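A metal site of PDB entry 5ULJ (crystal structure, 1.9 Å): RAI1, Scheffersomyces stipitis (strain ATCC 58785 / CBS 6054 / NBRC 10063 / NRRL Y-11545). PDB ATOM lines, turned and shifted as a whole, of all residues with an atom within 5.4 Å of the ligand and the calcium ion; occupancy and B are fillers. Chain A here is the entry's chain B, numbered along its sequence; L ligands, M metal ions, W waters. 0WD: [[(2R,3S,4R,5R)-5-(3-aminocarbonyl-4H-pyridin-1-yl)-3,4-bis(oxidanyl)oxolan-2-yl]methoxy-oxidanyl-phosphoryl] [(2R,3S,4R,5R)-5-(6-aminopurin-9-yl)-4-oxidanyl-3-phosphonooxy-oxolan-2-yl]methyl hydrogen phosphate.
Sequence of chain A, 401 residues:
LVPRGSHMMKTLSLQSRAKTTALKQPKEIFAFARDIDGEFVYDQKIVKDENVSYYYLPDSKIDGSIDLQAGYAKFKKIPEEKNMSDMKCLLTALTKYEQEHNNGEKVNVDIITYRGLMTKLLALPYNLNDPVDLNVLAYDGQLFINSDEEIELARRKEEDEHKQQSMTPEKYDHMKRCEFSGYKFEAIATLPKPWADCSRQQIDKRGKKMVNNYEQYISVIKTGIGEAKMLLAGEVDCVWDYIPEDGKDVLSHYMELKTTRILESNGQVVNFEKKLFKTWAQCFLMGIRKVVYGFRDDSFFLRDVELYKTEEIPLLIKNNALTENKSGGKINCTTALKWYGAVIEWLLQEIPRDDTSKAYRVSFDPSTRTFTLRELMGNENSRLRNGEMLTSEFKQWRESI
The calcium ion is bound by the side-chain carboxylate (OE2) of Glu 256 (2.4 Å), the side-chain carboxylate (OD2) of Asp 237 (2.4 Å), water W13 (2.5 Å), water W11 (2.5 Å), the backbone carbonyl oxygen (O) of Leu 257 (2.5 Å), an oxygen (OP2) of the ligand (2.5 Å) and water W9 (2.6 Å).
The calcium ion has seven donor atoms within binding distance.
The guanidinium group (NE) of Arg 115 is in salt-bridge range of an oxygen (O1A) of the ligand, 3.0 Å away.
The backbone carbonyl oxygen (O) of Asn 83 lies close to a nitrogen (N1N) of the ligand, 3.4 Å away.
O2N of the ligand is in hydrogen-bond range of N of Gly 116 (2.8 Å).
OE1 of Glu 235 lies close to O2B of the ligand, 3.5 Å away.
O1N of the ligand is in hydrogen-bond range of N of Glu 235, 2.8 Å away.
The side-chain amino group (NZ) of Lys 258 lies within salt-bridge range of an oxygen (OP1) of the ligand (3.0 Å).
The side-chain hydroxyl (OG) of Ser 147 sits at hydrogen-bond distance from a nitrogen (N7N) of the ligand, at 2.7 Å.
The side-chain amide nitrogen (NE2) of Gln 216 lies within hydrogen-bond range of an oxygen (O3M) of the ligand.
The side-chain amide nitrogen of Asn 83 lies close to a nitrogen (N6A) of the ligand, 3.0 Å away.
Residues that only touch the ligand: Ile 78 (3.999 Å), Glu 80 (3.6 Å), Met 84 (3.5 Å), Tyr 114 (3.6 Å), Glu 152 (3.6 Å), Tyr 183 (3.5 Å), Asn 213 (3.5 Å), Ala 233 (3.7 Å), Gly 234 (3.4 Å) and Gln 282 (3.7 Å).
Water W11 lies within hydrogen-bond range of O2B of the ligand (2.8 Å) and OD1 of Asp 237 (2.9 Å).
Water W3 lies within hydrogen-bond range of O3M of the ligand, OD1 of Asn 83 and NH1 of Arg 34.
Water W8 lies within hydrogen-bond range of O1A of the ligand (2.7 Å) and OG1 of Thr 119 (3.1 Å).
Water W5 lies within hydrogen-bond range of ND2 of Asn 213, O of Ile 78, NZ of Lys 77 and N1A of the ligand.
The side-chain amide nitrogen (ND2) of Asn 83 sits at hydrogen-bond distance from the side-chain carboxylate (OE2) of Glu 80.
O of Asn 213 lies within hydrogen-bond range of NH2 of Arg 34 (3.0 Å).
O of Arg 115 sits at hydrogen-bond distance from OG1 of Thr 119 (3.1 Å).
OD1 of Asn 213 is in hydrogen-bond range of N of Ile 78 (2.8 Å).
O of Glu 235 lies within hydrogen-bond range of NH2 of Arg 115.
The backbone carbonyl oxygen of Gln 216 sits at hydrogen-bond distance from the backbone NH of Arg 34, 2.9 Å away.
The side-chain carboxylate (OE2) of Glu 256 lies close to the side-chain amino group (NZ) of Lys 258, 3.4 Å away.
The side-chain amide oxygen (OE1) of Gln 282 lies within hydrogen-bond range of the side-chain amino group (NZ) of Lys 258 (2.7 Å).
Within 4 Å of the calcium ion: Asp 237, Glu 256 and Leu 257.
The nearest printed residue that does not touch the calcium ion is Lys 258 (4.2 Å).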
ATOM      1  N   ARG A  34      -0.058 -19.315 -30.766  1.00  0.00           N
ATOM      2  CA  ARG A  34      -0.856 -20.272 -30.013  1.00  0.00           C
ATOM      3  C   ARG A  34      -1.923 -20.851 -30.942  1.00  0.00           C
ATOM      4  O   ARG A  34      -2.566 -20.093 -31.676  1.00  0.00           O
ATOM      5  CB  ARG A  34      -1.495 -19.597 -28.798  1.00  0.00           C
ATOM      6  CG  ARG A  34      -2.300 -20.525 -27.906  1.00  0.00           C
ATOM      7  CD  ARG A  34      -2.788 -19.785 -26.660  1.00  0.00           C
ATOM      8  NE  ARG A  34      -3.713 -18.707 -26.993  1.00  0.00           N
ATOM      9  CZ  ARG A  34      -3.940 -17.651 -26.223  1.00  0.00           C
ATOM     10  NH1 ARG A  34      -3.300 -17.515 -25.070  1.00  0.00           N
ATOM     11  NH2 ARG A  34      -4.794 -16.711 -26.607  1.00  0.00           N
ATOM     12  N   LYS A  77     -13.757 -19.372 -26.018  1.00  0.00           N
ATOM     13  CA  LYS A  77     -13.015 -18.324 -25.313  1.00  0.00           C
ATOM     14  C   LYS A  77     -12.032 -18.909 -24.309  1.00  0.00           C
ATOM     15  O   LYS A  77     -12.412 -19.730 -23.461  1.00  0.00           O
ATOM     16  CB  LYS A  77     -13.992 -17.369 -24.631  1.00  0.00           C
ATOM     17  CG  LYS A  77     -13.339 -16.230 -23.861  1.00  0.00           C
ATOM     18  CD  LYS A  77     -14.414 -15.331 -23.255  1.00  0.00           C
ATOM     19  CE  LYS A  77     -13.823 -14.347 -22.251  1.00  0.00           C
ATOM     20  NZ  LYS A  77     -12.927 -13.349 -22.886  1.00  0.00           N
ATOM     21  N   ILE A  78     -10.780 -18.486 -24.381  1.00  0.00           N
ATOM     22  CA  ILE A  78      -9.741 -18.996 -23.496  1.00  0.00           C
ATOM     23  C   ILE A  78      -9.874 -18.389 -22.102  1.00  0.00           C
ATOM     24  O   ILE A  78     -10.157 -17.195 -21.959  1.00  0.00           O
ATOM     25  CB  ILE A  78      -8.321 -18.734 -24.079  1.00  0.00           C
ATOM     26  CG1 ILE A  78      -7.243 -19.484 -23.285  1.00  0.00           C
ATOM     27  CG2 ILE A  78      -8.015 -17.231 -24.157  1.00  0.00           C
ATOM     28  CD1 ILE A  78      -5.889 -19.498 -23.961  1.00  0.00           C
ATOM     29  N   GLU A  80      -9.036 -16.786 -18.438  1.00  0.00           N
ATOM     30  CA  GLU A  80      -8.126 -15.700 -18.063  1.00  0.00           C
ATOM     31  C   GLU A  80      -6.823 -16.231 -17.498  1.00  0.00           C
ATOM     32  O   GLU A  80      -5.767 -15.599 -17.635  1.00  0.00           O
ATOM     33  CB  GLU A  80      -8.800 -14.771 -17.050  1.00  0.00           C
ATOM     34  CG  GLU A  80      -9.059 -13.365 -17.572  1.00  0.00           C
ATOM     35  CD  GLU A  80      -7.778 -12.605 -17.868  1.00  0.00           C
ATOM     36  OE1 GLU A  80      -7.150 -12.109 -16.922  1.00  0.00           O
ATOM     37  OE2 GLU A  80      -7.421 -12.509 -19.057  1.00  0.00           O
ATOM     38  N   ASN A  83      -4.398 -16.577 -20.248  1.00  0.00           N
ATOM     39  CA  ASN A  83      -4.270 -15.394 -21.101  1.00  0.00           C
ATOM     40  C   ASN A  83      -2.835 -14.851 -21.107  1.00  0.00           C
ATOM     41  O   ASN A  83      -2.622 -13.642 -21.100  1.00  0.00           O
ATOM     42  CB  ASN A  83      -5.251 -14.306 -20.641  1.00  0.00           C
ATOM     43  CG  ASN A  83      -5.362 -13.160 -21.628  1.00  0.00           C
ATOM     44  OD1 ASN A  83      -5.163 -13.330 -22.833  1.00  0.00           O
ATOM     45  ND2 ASN A  83      -5.664 -11.966 -21.112  1.00  0.00           N
ATOM     46  N   MET A  84      -1.866 -15.756 -21.122  1.00  0.00           N
ATOM     47  CA  MET A  84      -0.440 -15.408 -21.126  1.00  0.00           C
ATOM     48  C   MET A  84      -0.114 -14.385 -20.037  1.00  0.00           C
ATOM     49  O   MET A  84       0.550 -13.379 -20.302  1.00  0.00           O
ATOM     50  CB  MET A  84      -0.043 -14.873 -22.505  1.00  0.00           C
ATOM     51  CG  MET A  84      -0.165 -15.895 -23.625  1.00  0.00           C
ATOM     52  SD  MET A  84       0.219 -15.229 -25.258  1.00  0.00           S
ATOM     53  CE  MET A  84       1.937 -14.758 -25.044  1.00  0.00           C
ATOM     54  N   SER A  85      -0.588 -14.657 -18.825  1.00  0.00           N
ATOM     55  CA  SER A  85      -0.383 -13.750 -17.702  1.00  0.00           C
ATOM     56  C   SER A  85       1.036 -13.820 -17.159  1.00  0.00           C
ATOM     57  O   SER A  85       1.474 -12.938 -16.422  1.00  0.00           O
ATOM     58  CB  SER A  85      -1.390 -14.038 -16.590  1.00  0.00           C
ATOM     59  OG  SER A  85      -2.713 -13.747 -17.006  1.00  0.00           O
ATOM     60  N   TYR A 114       5.641  -6.719 -22.833  1.00  0.00           N
ATOM     61  CA  TYR A 114       4.557  -6.833 -23.804  1.00  0.00           C
ATOM     62  C   TYR A 114       4.140  -5.457 -24.300  1.00  0.00           C
ATOM     63  O   TYR A 114       4.225  -4.470 -23.574  1.00  0.00           O
ATOM     64  CB  TYR A 114       3.353  -7.553 -23.199  1.00  0.00           C
ATOM     65  CG  TYR A 114       3.590  -8.994 -22.838  1.00  0.00           C
ATOM     66  CD1 TYR A 114       3.453 -10.001 -23.798  1.00  0.00           C
ATOM     67  CD2 TYR A 114       3.925  -9.372 -21.546  1.00  0.00           C
ATOM     68  CE1 TYR A 114       3.662 -11.333 -23.470  1.00  0.00           C
ATOM     69  CE2 TYR A 114       4.128 -10.689 -21.210  1.00  0.00           C
ATOM     70  CZ  TYR A 114       3.998 -11.665 -22.174  1.00  0.00           C
ATOM     71  OH  TYR A 114       4.198 -12.986 -21.847  1.00  0.00           O
ATOM     72  N   ARG A 115       3.672  -5.399 -25.550  1.00  0.00           N
ATOM     73  CA  ARG A 115       3.233  -4.150 -26.169  1.00  0.00           C
ATOM     74  C   ARG A 115       2.072  -3.523 -25.400  1.00  0.00           C
ATOM     75  O   ARG A 115       2.061  -2.317 -25.171  1.00  0.00           O
ATOM     76  CB  ARG A 115       2.830  -4.398 -27.630  1.00  0.00           C
ATOM     77  CG  ARG A 115       2.348  -3.162 -28.387  1.00  0.00           C
ATOM     78  CD  ARG A 115       0.830  -3.013 -28.342  1.00  0.00           C
ATOM     79  NE  ARG A 115       0.155  -4.296 -28.567  1.00  0.00           N
ATOM     80  CZ  ARG A 115      -0.140  -4.780 -29.768  1.00  0.00           C
ATOM     81  NH1 ARG A 115       0.182  -4.101 -30.857  1.00  0.00           N
ATOM     82  NH2 ARG A 115      -0.757  -5.953 -29.877  1.00  0.00           N
ATOM     83  N   GLY A 116       1.107  -4.344 -25.027  1.00  0.00           N
ATOM     84  CA  GLY A 116      -0.100  -3.872 -24.372  1.00  0.00           C
ATOM     85  C   GLY A 116       0.172  -3.143 -23.066  1.00  0.00           C
ATOM     86  O   GLY A 116      -0.533  -2.205 -22.719  1.00  0.00           O
ATOM     87  N   LEU A 117       1.205  -3.581 -22.368  1.00  0.00           N
ATOM     88  CA  LEU A 117       1.589  -2.959 -21.107  1.00  0.00           C
ATOM     89  C   LEU A 117       2.146  -1.558 -21.341  1.00  0.00           C
ATOM     90  O   LEU A 117       1.919  -0.650 -20.534  1.00  0.00           O
ATOM     91  CB  LEU A 117       2.614  -3.827 -20.370  1.00  0.00           C
ATOM     92  CG  LEU A 117       2.202  -5.279 -20.148  1.00  0.00           C
ATOM     93  CD1 LEU A 117       3.296  -6.043 -19.433  1.00  0.00           C
ATOM     94  CD2 LEU A 117       0.886  -5.360 -19.379  1.00  0.00           C
ATOM     95  N   THR A 119       1.323   0.230 -23.948  1.00  0.00           N
ATOM     96  CA  THR A 119       0.176   0.979 -24.431  1.00  0.00           C
ATOM     97  C   THR A 119      -0.541   1.660 -23.268  1.00  0.00           C
ATOM     98  O   THR A 119      -0.992   2.805 -23.373  1.00  0.00           O
ATOM     99  CB  THR A 119      -0.825   0.085 -25.190  1.00  0.00           C
ATOM    100  OG1 THR A 119      -0.176  -0.494 -26.333  1.00  0.00           O
ATOM    101  CG2 THR A 119      -2.032   0.879 -25.657  1.00  0.00           C
ATOM    102  N   ASN A 146       6.187  -6.875 -16.506  1.00  0.00           N
ATOM    103  CA  ASN A 146       4.967  -7.649 -16.683  1.00  0.00           C
ATOM    104  C   ASN A 146       3.865  -7.147 -15.760  1.00  0.00           C
ATOM    105  O   ASN A 146       4.146  -6.566 -14.717  1.00  0.00           O
ATOM    106  CB  ASN A 146       5.240  -9.136 -16.420  1.00  0.00           C
ATOM    107  CG  ASN A 146       4.115 -10.025 -16.917  1.00  0.00           C
ATOM    108  OD1 ASN A 146       3.442  -9.711 -17.896  1.00  0.00           O
ATOM    109  ND2 ASN A 146       3.915 -11.157 -16.241  1.00  0.00           N
ATOM    110  N   SER A 147       2.619  -7.342 -16.170  1.00  0.00           N
ATOM    111  CA  SER A 147       1.492  -7.104 -15.282  1.00  0.00           C
ATOM    112  C   SER A 147       1.537  -8.143 -14.164  1.00  0.00           C
ATOM    113  O   SER A 147       2.087  -9.226 -14.349  1.00  0.00           O
ATOM    114  CB  SER A 147       0.170  -7.181 -16.041  1.00  0.00           C
ATOM    115  OG  SER A 147       0.037  -8.420 -16.705  1.00  0.00           O
ATOM    116  N   GLU A 152      -4.092  -9.172 -11.708  1.00  0.00           N
ATOM    117  CA  GLU A 152      -4.849  -9.273 -12.957  1.00  0.00           C
ATOM    118  C   GLU A 152      -5.993 -10.288 -12.838  1.00  0.00           C
ATOM    119  O   GLU A 152      -7.111 -10.011 -13.269  1.00  0.00           O
ATOM    120  CB  GLU A 152      -3.939  -9.654 -14.118  1.00  0.00           C
ATOM    121  CG  GLU A 152      -2.975  -8.554 -14.556  1.00  0.00           C
ATOM    122  CD  GLU A 152      -3.696  -7.282 -14.953  1.00  0.00           C
ATOM    123  OE1 GLU A 152      -4.556  -7.335 -15.862  1.00  0.00           O
ATOM    124  OE2 GLU A 152      -3.409  -6.227 -14.353  1.00  0.00           O
ATOM    125  N   TYR A 183     -13.937 -10.489 -32.732  1.00  0.00           N
ATOM    126  CA  TYR A 183     -13.297 -11.706 -33.206  1.00  0.00           C
ATOM    127  C   TYR A 183     -14.009 -12.254 -34.441  1.00  0.00           C
ATOM    128  O   TYR A 183     -13.380 -12.852 -35.307  1.00  0.00           O
ATOM    129  CB  TYR A 183     -13.266 -12.755 -32.090  1.00  0.00           C
ATOM    130  CG  TYR A 183     -12.396 -12.379 -30.914  1.00  0.00           C
ATOM    131  CD1 TYR A 183     -11.012 -12.394 -31.008  1.00  0.00           C
ATOM    132  CD2 TYR A 183     -12.966 -12.019 -29.702  1.00  0.00           C
ATOM    133  CE1 TYR A 183     -10.219 -12.052 -29.927  1.00  0.00           C
ATOM    134  CE2 TYR A 183     -12.183 -11.674 -28.618  1.00  0.00           C
ATOM    135  CZ  TYR A 183     -10.808 -11.700 -28.738  1.00  0.00           C
ATOM    136  OH  TYR A 183     -10.019 -11.361 -27.665  1.00  0.00           O
ATOM    137  N   ASN A 213     -10.593 -17.144 -29.587  1.00  0.00           N
ATOM    138  CA  ASN A 213      -9.430 -16.310 -29.286  1.00  0.00           C
ATOM    139  C   ASN A 213      -8.270 -17.152 -28.760  1.00  0.00           C
ATOM    140  O   ASN A 213      -7.330 -16.632 -28.147  1.00  0.00           O
ATOM    141  CB  ASN A 213      -9.791 -15.205 -28.280  1.00  0.00           C
ATOM    142  CG  ASN A 213     -10.310 -15.733 -26.960  1.00  0.00           C
ATOM    143  OD1 ASN A 213     -10.346 -16.941 -26.726  1.00  0.00           O
ATOM    144  ND2 ASN A 213     -10.707 -14.821 -26.079  1.00  0.00           N
ATOM    145  N   GLN A 216      -3.736 -17.276 -31.813  1.00  0.00           N
ATOM    146  CA  GLN A 216      -3.146 -15.944 -31.770  1.00  0.00           C
ATOM    147  C   GLN A 216      -1.707 -15.938 -32.281  1.00  0.00           C
ATOM    148  O   GLN A 216      -0.915 -16.824 -31.963  1.00  0.00           O
ATOM    149  CB  GLN A 216      -3.207 -15.387 -30.349  1.00  0.00           C
ATOM    150  CG  GLN A 216      -4.287 -14.333 -30.169  1.00  0.00           C
ATOM    151  CD  GLN A 216      -4.389 -13.832 -28.734  1.00  0.00           C
ATOM    152  OE1 GLN A 216      -5.446 -13.893 -28.116  1.00  0.00           O
ATOM    153  NE2 GLN A 216      -3.269 -13.346 -28.209  1.00  0.00           N
ATOM    154  N   ILE A 218       1.804 -13.951 -32.380  1.00  0.00           N
ATOM    155  CA  ILE A 218       2.564 -12.970 -31.599  1.00  0.00           C
ATOM    156  C   ILE A 218       3.858 -12.566 -32.283  1.00  0.00           C
ATOM    157  O   ILE A 218       4.763 -13.386 -32.468  1.00  0.00           O
ATOM    158  CB  ILE A 218       2.900 -13.495 -30.192  1.00  0.00           C
ATOM    159  CG1 ILE A 218       1.649 -14.074 -29.523  1.00  0.00           C
ATOM    160  CG2 ILE A 218       3.523 -12.389 -29.352  1.00  0.00           C
ATOM    161  CD1 ILE A 218       0.532 -13.073 -29.319  1.00  0.00           C
ATOM    162  N   ALA A 233       6.663  -7.691 -27.269  1.00  0.00           N
ATOM    163  CA  ALA A 233       5.883  -8.786 -27.815  1.00  0.00           C
ATOM    164  C   ALA A 233       4.423  -8.351 -27.928  1.00  0.00           C
ATOM    165  O   ALA A 233       3.826  -7.912 -26.943  1.00  0.00           O
ATOM    166  CB  ALA A 233       6.020 -10.025 -26.960  1.00  0.00           C
ATOM    167  N   GLY A 234       3.857  -8.479 -29.124  1.00  0.00           N
ATOM    168  CA  GLY A 234       2.499  -8.032 -29.338  1.00  0.00           C
ATOM    169  C   GLY A 234       1.721  -8.896 -30.308  1.00  0.00           C
ATOM    170  O   GLY A 234       2.262  -9.387 -31.298  1.00  0.00           O
ATOM    171  N   GLU A 235       0.436  -9.086 -30.010  1.00  0.00           N
ATOM    172  CA  GLU A 235      -0.460  -9.816 -30.898  1.00  0.00           C
ATOM    173  C   GLU A 235      -0.666  -9.036 -32.193  1.00  0.00           C
ATOM    174  O   GLU A 235      -0.821  -7.821 -32.175  1.00  0.00           O
ATOM    175  CB  GLU A 235      -1.802 -10.076 -30.196  1.00  0.00           C
ATOM    176  CG  GLU A 235      -2.794 -10.916 -31.003  1.00  0.00           C
ATOM    177  CD  GLU A 235      -3.628 -10.097 -31.963  1.00  0.00           C
ATOM    178  OE1 GLU A 235      -3.702  -8.865 -31.789  1.00  0.00           O
ATOM    179  OE2 GLU A 235      -4.219 -10.688 -32.896  1.00  0.00           O
ATOM    180  N   ASP A 237      -3.021  -9.073 -35.774  1.00  0.00           N
ATOM    181  CA  ASP A 237      -4.251  -9.629 -36.332  1.00  0.00           C
ATOM    182  C   ASP A 237      -4.039 -10.348 -37.665  1.00  0.00           C
ATOM    183  O   ASP A 237      -4.430 -11.512 -37.805  1.00  0.00           O
ATOM    184  CB  ASP A 237      -5.297  -8.520 -36.518  1.00  0.00           C
ATOM    185  CG  ASP A 237      -5.934  -8.111 -35.208  1.00  0.00           C
ATOM    186  OD1 ASP A 237      -5.888  -8.897 -34.238  1.00  0.00           O
ATOM    187  OD2 ASP A 237      -6.502  -6.991 -35.145  1.00  0.00           O
ATOM    188  N   GLU A 256      -3.931  -3.975 -38.234  1.00  0.00           N
ATOM    189  CA  GLU A 256      -4.777  -4.151 -37.057  1.00  0.00           C
ATOM    190  C   GLU A 256      -6.251  -4.094 -37.414  1.00  0.00           C
ATOM    191  O   GLU A 256      -6.670  -3.252 -38.209  1.00  0.00           O
ATOM    192  CB  GLU A 256      -4.434  -3.085 -36.016  1.00  0.00           C
ATOM    193  CG  GLU A 256      -5.364  -3.045 -34.813  1.00  0.00           C
ATOM    194  CD  GLU A 256      -5.179  -4.242 -33.902  1.00  0.00           C
ATOM    195  OE1 GLU A 256      -4.088  -4.858 -33.930  1.00  0.00           O
ATOM    196  OE2 GLU A 256      -6.123  -4.577 -33.161  1.00  0.00           O
ATOM    197  N   LEU A 257      -7.042  -4.991 -36.825  1.00  0.00           N
ATOM    198  CA  LEU A 257      -8.487  -5.014 -37.058  1.00  0.00           C
ATOM    199  C   LEU A 257      -9.262  -4.627 -35.802  1.00  0.00           C
ATOM    200  O   LEU A 257      -9.012  -5.165 -34.723  1.00  0.00           O
ATOM    201  CB  LEU A 257      -8.939  -6.389 -37.547  1.00  0.00           C
ATOM    202  CG  LEU A 257      -8.369  -6.878 -38.880  1.00  0.00           C
ATOM    203  CD1 LEU A 257      -8.928  -8.247 -39.228  1.00  0.00           C
ATOM    204  CD2 LEU A 257      -8.662  -5.883 -39.977  1.00  0.00           C
ATOM    205  N   LYS A 258     -10.193  -3.692 -35.939  1.00  0.00           N
ATOM    206  CA  LYS A 258     -11.017  -3.242 -34.826  1.00  0.00           C
ATOM    207  C   LYS A 258     -12.494  -3.192 -35.225  1.00  0.00           C
ATOM    208  O   LYS A 258     -12.820  -3.063 -36.409  1.00  0.00           O
ATOM    209  CB  LYS A 258     -10.563  -1.858 -34.341  1.00  0.00           C
ATOM    210  CG  LYS A 258      -9.143  -1.795 -33.819  1.00  0.00           C
ATOM    211  CD  LYS A 258      -9.012  -2.473 -32.456  1.00  0.00           C
ATOM    212  CE  LYS A 258      -7.674  -2.156 -31.821  1.00  0.00           C
ATOM    213  NZ  LYS A 258      -7.467  -2.930 -30.562  1.00  0.00           N
ATOM    214  N   GLN A 282      -1.547   1.521 -29.566  1.00  0.00           N
ATOM    215  CA  GLN A 282      -1.290   0.091 -29.730  1.00  0.00           C
ATOM    216  C   GLN A 282      -0.471  -0.192 -30.988  1.00  0.00           C
ATOM    217  O   GLN A 282       0.470  -0.987 -30.957  1.00  0.00           O
ATOM    218  CB  GLN A 282      -2.619  -0.672 -29.779  1.00  0.00           C
ATOM    219  CG  GLN A 282      -2.468  -2.163 -30.005  1.00  0.00           C
ATOM    220  CD  GLN A 282      -3.803  -2.871 -30.154  1.00  0.00           C
ATOM    221  OE1 GLN A 282      -4.862  -2.232 -30.067  1.00  0.00           O
ATOM    222  NE2 GLN A 282      -3.769  -4.174 -30.376  1.00  0.00           N
HETATM  223  O7N 0WD L   1      -3.993  -9.313 -19.437  1.00  0.00           O
HETATM  224  C7N 0WD L   1      -2.782  -9.183 -19.285  1.00  0.00           C
HETATM  225  N7N 0WD L   1      -2.220  -8.608 -18.220  1.00  0.00           N
HETATM  226  C3N 0WD L   1      -1.882  -9.629 -20.245  1.00  0.00           C
HETATM  227  C2N 0WD L   1      -2.351 -10.249 -21.395  1.00  0.00           C
HETATM  228  C4N 0WD L   1      -0.521  -9.452 -20.053  1.00  0.00           C
HETATM  229  C5N 0WD L   1       0.384  -9.885 -21.009  1.00  0.00           C
HETATM  230  C6N 0WD L   1      -0.077 -10.517 -22.157  1.00  0.00           C
HETATM  231  N1N 0WD L   1      -1.440 -10.697 -22.358  1.00  0.00           N
HETATM  232  C1M 0WD L   1      -1.906 -11.370 -23.602  1.00  0.00           C
HETATM  233  C2M 0WD L   1      -2.737 -10.458 -24.475  1.00  0.00           C
HETATM  234  O2M 0WD L   1      -4.065 -10.289 -23.939  1.00  0.00           O
HETATM  235  C3M 0WD L   1      -2.744 -11.339 -25.672  1.00  0.00           C
HETATM  236  O3M 0WD L   1      -3.375 -12.580 -25.337  1.00  0.00           O
HETATM  237  O4M 0WD L   1      -0.747 -11.632 -24.437  1.00  0.00           O
HETATM  238  C4M 0WD L   1      -1.237 -11.560 -25.810  1.00  0.00           C
HETATM  239  C5M 0WD L   1      -0.560 -10.392 -26.555  1.00  0.00           C
HETATM  240  O5M 0WD L   1      -0.200  -9.323 -25.681  1.00  0.00           O
HETATM  241  PN  0WD L   1      -0.489  -7.798 -26.136  1.00  0.00           P
HETATM  242  O1N 0WD L   1      -0.412  -8.027 -27.603  1.00  0.00           O
HETATM  243  O2N 0WD L   1       0.543  -7.091 -25.347  1.00  0.00           O
HETATM  244  O3P 0WD L   1      -2.006  -7.505 -25.681  1.00  0.00           O
HETATM  245  PA  0WD L   1      -2.897  -6.213 -26.021  1.00  0.00           P
HETATM  246  O1A 0WD L   1      -2.115  -5.290 -26.879  1.00  0.00           O
HETATM  247  O2A 0WD L   1      -3.475  -5.711 -24.760  1.00  0.00           O
HETATM  248  O5B 0WD L   1      -4.089  -6.839 -26.907  1.00  0.00           O
HETATM  249  C5B 0WD L   1      -3.879  -7.240 -28.264  1.00  0.00           C
HETATM  250  C4B 0WD L   1      -4.796  -8.418 -28.599  1.00  0.00           C
HETATM  251  C3B 0WD L   1      -6.245  -8.027 -28.460  1.00  0.00           C
HETATM  252  O3B 0WD L   1      -6.656  -7.185 -29.555  1.00  0.00           O
HETATM  253  P2' 0WD L   1      -7.680  -5.985 -29.328  1.00  0.00           P
HETATM  254  OP2 0WD L   1      -7.939  -5.561 -30.724  1.00  0.00           O
HETATM  255  OP1 0WD L   1      -6.917  -5.010 -28.534  1.00  0.00           O
HETATM  256  OP3 0WD L   1      -8.836  -6.608 -28.666  1.00  0.00           O
HETATM  257  O4B 0WD L   1      -4.670  -9.440 -27.576  1.00  0.00           O
HETATM  258  C1B 0WD L   1      -5.941 -10.145 -27.579  1.00  0.00           C
HETATM  259  C2B 0WD L   1      -6.806  -9.412 -28.619  1.00  0.00           C
HETATM  260  O2B 0WD L   1      -6.456  -9.879 -29.922  1.00  0.00           O
HETATM  261  N9A 0WD L   1      -6.482 -10.082 -26.190  1.00  0.00           N
HETATM  262  C4A 0WD L   1      -6.980 -11.144 -25.567  1.00  0.00           C
HETATM  263  N3A 0WD L   1      -7.127 -12.418 -25.960  1.00  0.00           N
HETATM  264  C2A 0WD L   1      -7.698 -13.357 -25.095  1.00  0.00           C
HETATM  265  N1A 0WD L   1      -8.088 -12.925 -23.831  1.00  0.00           N
HETATM  266  C5A 0WD L   1      -7.373 -10.765 -24.349  1.00  0.00           C
HETATM  267  C6A 0WD L   1      -7.916 -11.641 -23.508  1.00  0.00           C
HETATM  268  N6A 0WD L   1      -8.277 -11.176 -22.314  1.00  0.00           N
HETATM  269  N7A 0WD L   1      -7.108  -9.467 -24.226  1.00  0.00           N
HETATM  270  C8A 0WD L   1      -6.556  -9.045 -25.356  1.00  0.00           C
HETATM  271 CA    CA M   1      -7.633  -6.402 -33.071  1.00  0.00          CA
HETATM  272  O   HOH W   1      -4.755  -8.236 -22.434  1.00  0.00           O
HETATM  273  O   HOH W   2      -2.346  -6.312 -22.104  1.00  0.00           O
HETATM  274  O   HOH W   3      -4.044 -14.719 -24.458  1.00  0.00           O
HETATM  275  O   HOH W   4      -6.309  -5.347 -24.498  1.00  0.00           O
HETATM  276  O   HOH W   5     -10.408 -14.699 -23.342  1.00  0.00           O
HETATM  277  O   HOH W   6      -9.151  -7.948 -26.653  1.00  0.00           O
HETATM  278  O   HOH W   7      -6.255  -9.516 -17.841  1.00  0.00           O
HETATM  279  O   HOH W   8      -2.403  -2.646 -26.595  1.00  0.00           O
HETATM  280  O   HOH W   9      -5.265  -6.702 -32.053  1.00  0.00           O
HETATM  281  O   HOH W  10      -0.004  -6.885 -22.473  1.00  0.00           O
HETATM  282  O   HOH W  11      -7.714  -8.657 -32.059  1.00  0.00           O
HETATM  283  O   HOH W  12       1.853 -11.451 -18.837  1.00  0.00           O
HETATM  284  O   HOH W  13      -9.993  -7.099 -33.237  1.00  0.00           O
